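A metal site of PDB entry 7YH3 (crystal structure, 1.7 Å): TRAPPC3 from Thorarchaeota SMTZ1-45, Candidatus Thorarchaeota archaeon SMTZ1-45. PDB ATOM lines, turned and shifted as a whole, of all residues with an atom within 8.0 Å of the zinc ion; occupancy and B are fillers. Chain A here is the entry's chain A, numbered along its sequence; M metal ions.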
ATOM      1  N   TYR A  15      21.795  17.279 -13.742  1.00  0.00           N
ATOM      2  CA  TYR A  15      22.861  17.767 -12.881  1.00  0.00           C
ATOM      3  C   TYR A  15      23.184  16.768 -11.770  1.00  0.00           C
ATOM      4  O   TYR A  15      24.351  16.612 -11.409  1.00  0.00           O
ATOM      5  CB  TYR A  15      22.483  19.122 -12.266  1.00  0.00           C
ATOM      6  CG  TYR A  15      23.601  19.718 -11.438  1.00  0.00           C
ATOM      7  CD1 TYR A  15      24.844  19.972 -11.993  1.00  0.00           C
ATOM      8  CD2 TYR A  15      23.411  20.016 -10.092  1.00  0.00           C
ATOM      9  CE1 TYR A  15      25.879  20.519 -11.252  1.00  0.00           C
ATOM     10  CE2 TYR A  15      24.441  20.566  -9.329  1.00  0.00           C
ATOM     11  CZ  TYR A  15      25.667  20.812  -9.915  1.00  0.00           C
ATOM     12  OH  TYR A  15      26.695  21.354  -9.184  1.00  0.00           O
ATOM     13  N   TYR A  75      20.552  36.660 -12.279  1.00  0.00           N
ATOM     14  CA  TYR A  75      19.730  35.686 -11.566  1.00  0.00           C
ATOM     15  C   TYR A  75      18.295  35.702 -12.069  1.00  0.00           C
ATOM     16  O   TYR A  75      17.680  34.639 -12.255  1.00  0.00           O
ATOM     17  CB  TYR A  75      19.792  35.955 -10.058  1.00  0.00           C
ATOM     18  CG  TYR A  75      19.813  34.709  -9.209  1.00  0.00           C
ATOM     19  CD1 TYR A  75      21.002  34.013  -8.995  1.00  0.00           C
ATOM     20  CD2 TYR A  75      18.648  34.205  -8.626  1.00  0.00           C
ATOM     21  CE1 TYR A  75      21.031  32.868  -8.219  1.00  0.00           C
ATOM     22  CE2 TYR A  75      18.669  33.055  -7.861  1.00  0.00           C
ATOM     23  CZ  TYR A  75      19.857  32.390  -7.662  1.00  0.00           C
ATOM     24  OH  TYR A  75      19.885  31.247  -6.896  1.00  0.00           O
ATOM     25  N   ASP A  99      19.918  32.245  -1.813  1.00  0.00           N
ATOM     26  CA  ASP A  99      18.710  31.743  -2.463  1.00  0.00           C
ATOM     27  C   ASP A  99      18.128  30.653  -1.584  1.00  0.00           C
ATOM     28  O   ASP A  99      18.820  29.684  -1.247  1.00  0.00           O
ATOM     29  CB  ASP A  99      19.022  31.205  -3.865  1.00  0.00           C
ATOM     30  CG  ASP A  99      17.778  30.916  -4.685  1.00  0.00           C
ATOM     31  OD1 ASP A  99      16.655  31.025  -4.139  1.00  0.00           O
ATOM     32  OD2 ASP A  99      17.922  30.573  -5.874  1.00  0.00           O
ATOM     33  N   ASP A 100      16.861  30.810  -1.183  1.00  0.00           N
ATOM     34  CA  ASP A 100      16.219  29.849  -0.306  1.00  0.00           C
ATOM     35  C   ASP A 100      15.556  28.708  -1.055  1.00  0.00           C
ATOM     36  O   ASP A 100      15.141  27.737  -0.410  1.00  0.00           O
ATOM     37  CB  ASP A 100      15.184  30.561   0.586  1.00  0.00           C
ATOM     38  CG  ASP A 100      14.079  31.220  -0.212  1.00  0.00           C
ATOM     39  OD1 ASP A 100      14.267  31.444  -1.427  1.00  0.00           O
ATOM     40  OD2 ASP A 100      13.026  31.537   0.379  1.00  0.00           O
ATOM     41  N   ASN A 101      15.428  28.806  -2.375  1.00  0.00           N
ATOM     42  CA  ASN A 101      14.866  27.745  -3.197  1.00  0.00           C
ATOM     43  C   ASN A 101      15.733  27.569  -4.443  1.00  0.00           C
ATOM     44  O   ASN A 101      15.297  27.722  -5.579  1.00  0.00           O
ATOM     45  CB  ASN A 101      13.412  28.043  -3.562  1.00  0.00           C
ATOM     46  CG  ASN A 101      12.712  26.834  -4.149  1.00  0.00           C
ATOM     47  OD1 ASN A 101      12.978  25.688  -3.767  1.00  0.00           O
ATOM     48  ND2 ASN A 101      11.810  27.071  -5.104  1.00  0.00           N
ATOM     49  N   CYS A 102      17.002  27.243  -4.204  1.00  0.00           N
ATOM     50  CA  CYS A 102      17.959  26.970  -5.281  1.00  0.00           C
ATOM     51  C   CYS A 102      17.432  25.903  -6.218  1.00  0.00           C
ATOM     52  O   CYS A 102      16.970  24.849  -5.780  1.00  0.00           O
ATOM     53  CB  CYS A 102      19.283  26.527  -4.659  1.00  0.00           C
ATOM     54  SG  CYS A 102      20.574  26.032  -5.802  1.00  0.00           S
ATOM     55  N   VAL A 103      17.501  26.171  -7.519  1.00  0.00           N
ATOM     56  CA  VAL A 103      16.985  25.193  -8.470  1.00  0.00           C
ATOM     57  C   VAL A 103      17.832  23.917  -8.469  1.00  0.00           C
ATOM     58  O   VAL A 103      17.303  22.825  -8.656  1.00  0.00           O
ATOM     59  CB  VAL A 103      16.890  25.793  -9.889  1.00  0.00           C
ATOM     60  CG1 VAL A 103      18.273  26.093 -10.454  1.00  0.00           C
ATOM     61  CG2 VAL A 103      16.141  24.845 -10.819  1.00  0.00           C
ATOM     62  N   TRP A 104      19.136  24.034  -8.207  1.00  0.00           N
ATOM     63  CA  TRP A 104      20.024  22.883  -8.409  1.00  0.00           C
ATOM     64  C   TRP A 104      19.777  21.769  -7.394  1.00  0.00           C
ATOM     65  O   TRP A 104      19.821  20.583  -7.740  1.00  0.00           O
ATOM     66  CB  TRP A 104      21.485  23.340  -8.367  1.00  0.00           C
ATOM     67  CG  TRP A 104      21.807  24.444  -9.327  1.00  0.00           C
ATOM     68  CD1 TRP A 104      21.934  25.779  -9.035  1.00  0.00           C
ATOM     69  CD2 TRP A 104      22.061  24.315 -10.727  1.00  0.00           C
ATOM     70  NE1 TRP A 104      22.230  26.478 -10.175  1.00  0.00           N
ATOM     71  CE2 TRP A 104      22.316  25.611 -11.227  1.00  0.00           C
ATOM     72  CE3 TRP A 104      22.076  23.228 -11.613  1.00  0.00           C
ATOM     73  CZ2 TRP A 104      22.602  25.852 -12.568  1.00  0.00           C
ATOM     74  CZ3 TRP A 104      22.348  23.467 -12.943  1.00  0.00           C
ATOM     75  CH2 TRP A 104      22.619  24.771 -13.412  1.00  0.00           C
ATOM     76  N   CYS A 105      19.502  22.121  -6.143  1.00  0.00           N
ATOM     77  CA  CYS A 105      19.483  21.140  -5.067  1.00  0.00           C
ATOM     78  C   CYS A 105      18.084  20.859  -4.527  1.00  0.00           C
ATOM     79  O   CYS A 105      17.953  20.404  -3.382  1.00  0.00           O
ATOM     80  CB  CYS A 105      20.410  21.576  -3.941  1.00  0.00           C
ATOM     81  SG  CYS A 105      19.986  23.173  -3.204  1.00  0.00           S
ATOM     82  N   GLN A 106      17.038  21.118  -5.305  1.00  0.00           N
ATOM     83  CA  GLN A 106      15.683  20.847  -4.849  1.00  0.00           C
ATOM     84  C   GLN A 106      15.525  19.382  -4.439  1.00  0.00           C
ATOM     85  O   GLN A 106      15.848  18.485  -5.217  1.00  0.00           O
ATOM     86  CB  GLN A 106      14.666  21.187  -5.929  1.00  0.00           C
ATOM     87  CG  GLN A 106      14.571  22.654  -6.291  1.00  0.00           C
ATOM     88  CD  GLN A 106      13.724  22.875  -7.529  1.00  0.00           C
ATOM     89  OE1 GLN A 106      12.507  23.065  -7.441  1.00  0.00           O
ATOM     90  NE2 GLN A 106      14.359  22.847  -8.689  1.00  0.00           N
ATOM     91  N   VAL A 108      17.176  17.577  -2.542  1.00  0.00           N
ATOM     92  CA  VAL A 108      18.440  16.857  -2.389  1.00  0.00           C
ATOM     93  C   VAL A 108      18.836  16.913  -0.924  1.00  0.00           C
ATOM     94  O   VAL A 108      18.965  17.997  -0.344  1.00  0.00           O
ATOM     95  CB  VAL A 108      19.541  17.437  -3.289  1.00  0.00           C
ATOM     96  CG1 VAL A 108      20.843  16.648  -3.111  1.00  0.00           C
ATOM     97  CG2 VAL A 108      19.108  17.445  -4.749  1.00  0.00           C
ATOM     98  N   GLY A 117      30.122  21.601  -1.862  1.00  0.00           N
ATOM     99  CA  GLY A 117      29.235  22.547  -2.496  1.00  0.00           C
ATOM    100  C   GLY A 117      28.494  21.917  -3.651  1.00  0.00           C
ATOM    101  O   GLY A 117      28.914  22.030  -4.811  1.00  0.00           O
ATOM    102  N   TYR A 118      27.385  21.238  -3.352  1.00  0.00           N
ATOM    103  CA  TYR A 118      26.612  20.536  -4.365  1.00  0.00           C
ATOM    104  C   TYR A 118      26.278  21.429  -5.558  1.00  0.00           C
ATOM    105  O   TYR A 118      26.216  20.943  -6.689  1.00  0.00           O
ATOM    106  CB  TYR A 118      25.323  19.981  -3.744  1.00  0.00           C
ATOM    107  CG  TYR A 118      24.456  19.179  -4.689  1.00  0.00           C
ATOM    108  CD1 TYR A 118      23.488  19.800  -5.473  1.00  0.00           C
ATOM    109  CD2 TYR A 118      24.604  17.803  -4.793  1.00  0.00           C
ATOM    110  CE1 TYR A 118      22.696  19.058  -6.350  1.00  0.00           C
ATOM    111  CE2 TYR A 118      23.821  17.064  -5.650  1.00  0.00           C
ATOM    112  CZ  TYR A 118      22.859  17.692  -6.433  1.00  0.00           C
ATOM    113  OH  TYR A 118      22.089  16.953  -7.291  1.00  0.00           O
ATOM    114  N   CYS A 119      26.111  22.723  -5.326  1.00  0.00           N
ATOM    115  CA  CYS A 119      25.646  23.680  -6.334  1.00  0.00           C
ATOM    116  C   CYS A 119      26.765  24.589  -6.854  1.00  0.00           C
ATOM    117  O   CYS A 119      26.496  25.703  -7.294  1.00  0.00           O
ATOM    118  CB  CYS A 119      24.510  24.519  -5.767  1.00  0.00           C
ATOM    119  SG  CYS A 119      23.492  23.648  -4.552  1.00  0.00           S
ATOM    120  N   GLU A 120      28.023  24.117  -6.826  1.00  0.00           N
ATOM    121  CA  GLU A 120      29.149  24.938  -7.263  1.00  0.00           C
ATOM    122  C   GLU A 120      29.147  25.217  -8.770  1.00  0.00           C
ATOM    123  O   GLU A 120      29.858  26.127  -9.233  1.00  0.00           O
ATOM    124  CB  GLU A 120      30.462  24.266  -6.869  1.00  0.00           C
ATOM    125  CG  GLU A 120      30.809  24.395  -5.377  1.00  0.00           C
ATOM    126  CD  GLU A 120      31.542  25.689  -5.041  1.00  0.00           C
ATOM    127  OE1 GLU A 120      31.597  26.580  -5.913  1.00  0.00           O
ATOM    128  OE2 GLU A 120      32.064  25.806  -3.920  1.00  0.00           O
ATOM    129  N   PHE A 122      26.969  26.755 -10.235  1.00  0.00           N
ATOM    130  CA  PHE A 122      26.566  28.145 -10.356  1.00  0.00           C
ATOM    131  C   PHE A 122      27.708  29.093 -10.044  1.00  0.00           C
ATOM    132  O   PHE A 122      27.784  30.182 -10.634  1.00  0.00           O
ATOM    133  CB  PHE A 122      25.376  28.458  -9.460  1.00  0.00           C
ATOM    134  CG  PHE A 122      24.909  29.881  -9.570  1.00  0.00           C
ATOM    135  CD1 PHE A 122      24.316  30.335 -10.739  1.00  0.00           C
ATOM    136  CD2 PHE A 122      25.064  30.766  -8.521  1.00  0.00           C
ATOM    137  CE1 PHE A 122      23.893  31.644 -10.854  1.00  0.00           C
ATOM    138  CE2 PHE A 122      24.642  32.073  -8.626  1.00  0.00           C
ATOM    139  CZ  PHE A 122      24.057  32.520  -9.796  1.00  0.00           C
ATOM    140  N   GLN A 141      30.917  28.378  -3.333  1.00  0.00           N
ATOM    141  CA  GLN A 141      29.655  28.178  -2.614  1.00  0.00           C
ATOM    142  C   GLN A 141      29.927  28.198  -1.117  1.00  0.00           C
ATOM    143  O   GLN A 141      30.705  27.376  -0.604  1.00  0.00           O
ATOM    144  CB  GLN A 141      28.997  26.862  -3.019  1.00  0.00           C
ATOM    145  CG  GLN A 141      27.780  26.546  -2.183  1.00  0.00           C
ATOM    146  CD  GLN A 141      26.808  25.653  -2.924  1.00  0.00           C
ATOM    147  OE1 GLN A 141      27.233  24.761  -3.657  1.00  0.00           O
ATOM    148  NE2 GLN A 141      25.523  25.917  -2.776  1.00  0.00           N
ATOM    149  N   MET A 143      27.443  27.874   1.304  1.00  0.00           N
ATOM    150  CA  MET A 143      26.722  26.748   1.879  1.00  0.00           C
ATOM    151  C   MET A 143      25.615  26.297   0.936  1.00  0.00           C
ATOM    152  O   MET A 143      25.190  27.029   0.045  1.00  0.00           O
ATOM    153  CB  MET A 143      26.151  27.078   3.267  1.00  0.00           C
ATOM    154  CG  MET A 143      25.281  28.313   3.331  1.00  0.00           C
ATOM    155  SD  MET A 143      24.921  28.702   5.054  1.00  0.00           S
ATOM    156  CE  MET A 143      23.708  30.012   4.869  1.00  0.00           C
ATOM    157  N   SER A 144      25.137  25.073   1.169  1.00  0.00           N
ATOM    158  CA  SER A 144      24.146  24.424   0.323  1.00  0.00           C
ATOM    159  C   SER A 144      23.065  23.788   1.181  1.00  0.00           C
ATOM    160  O   SER A 144      23.354  23.133   2.188  1.00  0.00           O
ATOM    161  CB  SER A 144      24.792  23.348  -0.562  1.00  0.00           C
ATOM    162  OG  SER A 144      23.836  22.720  -1.406  1.00  0.00           O
ATOM    163  N   LYS A 145      21.803  23.972   0.780  1.00  0.00           N
ATOM    164  CA  LYS A 145      20.709  23.249   1.418  1.00  0.00           C
ATOM    165  C   LYS A 145      20.825  21.749   1.210  1.00  0.00           C
ATOM    166  O   LYS A 145      20.288  20.976   2.014  1.00  0.00           O
ATOM    167  CB  LYS A 145      19.369  23.781   0.896  1.00  0.00           C
ATOM    168  CG  LYS A 145      18.159  23.256   1.661  1.00  0.00           C
ATOM    169  CD  LYS A 145      16.981  24.217   1.600  1.00  0.00           C
ATOM    170  CE  LYS A 145      16.403  24.304   0.206  1.00  0.00           C
ATOM    171  NZ  LYS A 145      15.185  25.162   0.159  1.00  0.00           N
ATOM    172  N   ALA A 146      21.517  21.326   0.152  1.00  0.00           N
ATOM    173  CA  ALA A 146      21.721  19.898  -0.088  1.00  0.00           C
ATOM    174  C   ALA A 146      22.480  19.228   1.048  1.00  0.00           C
ATOM    175  O   ALA A 146      22.298  18.034   1.287  1.00  0.00           O
ATOM    176  CB  ALA A 146      22.464  19.684  -1.405  1.00  0.00           C
ATOM    177  N   THR A 147      23.318  19.974   1.760  1.00  0.00           N
ATOM    178  CA  THR A 147      24.120  19.409   2.841  1.00  0.00           C
ATOM    179  C   THR A 147      23.640  19.819   4.230  1.00  0.00           C
ATOM    180  O   THR A 147      24.371  19.648   5.209  1.00  0.00           O
ATOM    181  CB  THR A 147      25.590  19.786   2.663  1.00  0.00           C
ATOM    182  OG1 THR A 147      25.724  21.208   2.655  1.00  0.00           O
ATOM    183  CG2 THR A 147      26.127  19.224   1.354  1.00  0.00           C
ATOM    184  N   VAL A 151      19.536  27.553   3.466  1.00  0.00           N
ATOM    185  CA  VAL A 151      19.554  28.237   2.179  1.00  0.00           C
ATOM    186  C   VAL A 151      20.862  27.896   1.463  1.00  0.00           C
ATOM    187  O   VAL A 151      21.767  27.281   2.028  1.00  0.00           O
ATOM    188  CB  VAL A 151      19.413  29.771   2.323  1.00  0.00           C
ATOM    189  CG1 VAL A 151      18.028  30.142   2.846  1.00  0.00           C
ATOM    190  CG2 VAL A 151      20.488  30.298   3.242  1.00  0.00           C
ATOM    191  N   CYS A 152      20.951  28.322   0.203  1.00  0.00           N
ATOM    192  CA  CYS A 152      22.187  28.256  -0.556  1.00  0.00           C
ATOM    193  C   CYS A 152      22.814  29.637  -0.636  1.00  0.00           C
ATOM    194  O   CYS A 152      22.122  30.633  -0.855  1.00  0.00           O
ATOM    195  CB  CYS A 152      21.925  27.707  -1.963  1.00  0.00           C
ATOM    196  SG  CYS A 152      21.291  26.018  -1.973  1.00  0.00           S
ATOM    197  N   VAL A 153      24.130  29.695  -0.437  1.00  0.00           N
ATOM    198  CA  VAL A 153      24.870  30.955  -0.446  1.00  0.00           C
ATOM    199  C   VAL A 153      26.148  30.767  -1.242  1.00  0.00           C
ATOM    200  O   VAL A 153      26.927  29.834  -0.976  1.00  0.00           O
ATOM    201  CB  VAL A 153      25.198  31.451   0.976  1.00  0.00           C
ATOM    202  CG1 VAL A 153      26.091  32.681   0.910  1.00  0.00           C
ATOM    203  CG2 VAL A 153      23.921  31.758   1.723  1.00  0.00           C
ATOM    204  N   TRP A 154      26.374  31.669  -2.205  1.00  0.00           N
ATOM    205  CA  TRP A 154      27.575  31.758  -3.024  1.00  0.00           C
ATOM    206  C   TRP A 154      28.278  33.072  -2.713  1.00  0.00           C
ATOM    207  O   TRP A 154      27.636  34.111  -2.560  1.00  0.00           O
ATOM    208  CB  TRP A 154      27.255  31.687  -4.517  1.00  0.00           C
ATOM    209  CG  TRP A 154      26.501  30.441  -4.954  1.00  0.00           C
ATOM    210  CD1 TRP A 154      27.046  29.284  -5.429  1.00  0.00           C
ATOM    211  CD2 TRP A 154      25.085  30.264  -4.985  1.00  0.00           C
ATOM    212  NE1 TRP A 154      26.052  28.387  -5.742  1.00  0.00           N
ATOM    213  CE2 TRP A 154      24.839  28.960  -5.477  1.00  0.00           C
ATOM    214  CE3 TRP A 154      24.000  31.068  -4.644  1.00  0.00           C
ATOM    215  CZ2 TRP A 154      23.550  28.446  -5.623  1.00  0.00           C
ATOM    216  CZ3 TRP A 154      22.711  30.554  -4.790  1.00  0.00           C
ATOM    217  CH2 TRP A 154      22.499  29.259  -5.283  1.00  0.00           C
HETATM  218 ZN    ZN M   1      21.465  24.856  -4.058  1.00  0.00          ZN
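N of Asp 99 is in hydrogen-bond range of O of Cys 152, at 2.9 Å. The side-chain sulfur of Cys 102 sits close to the backbone NH of Trp 104 (3.4 Å). The side-chain amide oxygen of Gln 141 sits at hydrogen-bond distance from the backbone NH of Cys 119, 2.9 Å away. SG of Cys 152 sits close to N of Lys 145 (3.5 Å). O of Cys 119 sits at hydrogen-bond distance from NE1 of Trp 154 (3.1 Å). SG of Cys 119 sits close to OG of Ser 144 (3.3 Å).
Within 4 Å of the zinc ion: Cys 102, Cys 105, Cys 119 and Cys 152. The nearest printed residue that does not touch the zinc ion is Ser 144 (4.1 Å).
SG of Cys 102 is bound to the zinc ion. SG of Cys 152 binds the zinc ion (2.4 Å). The side-chain sulfur (SG) of Cys 105 is bound to the zinc ion. The zinc ion is bound by SG of Cys 119, 2.4 Å away.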
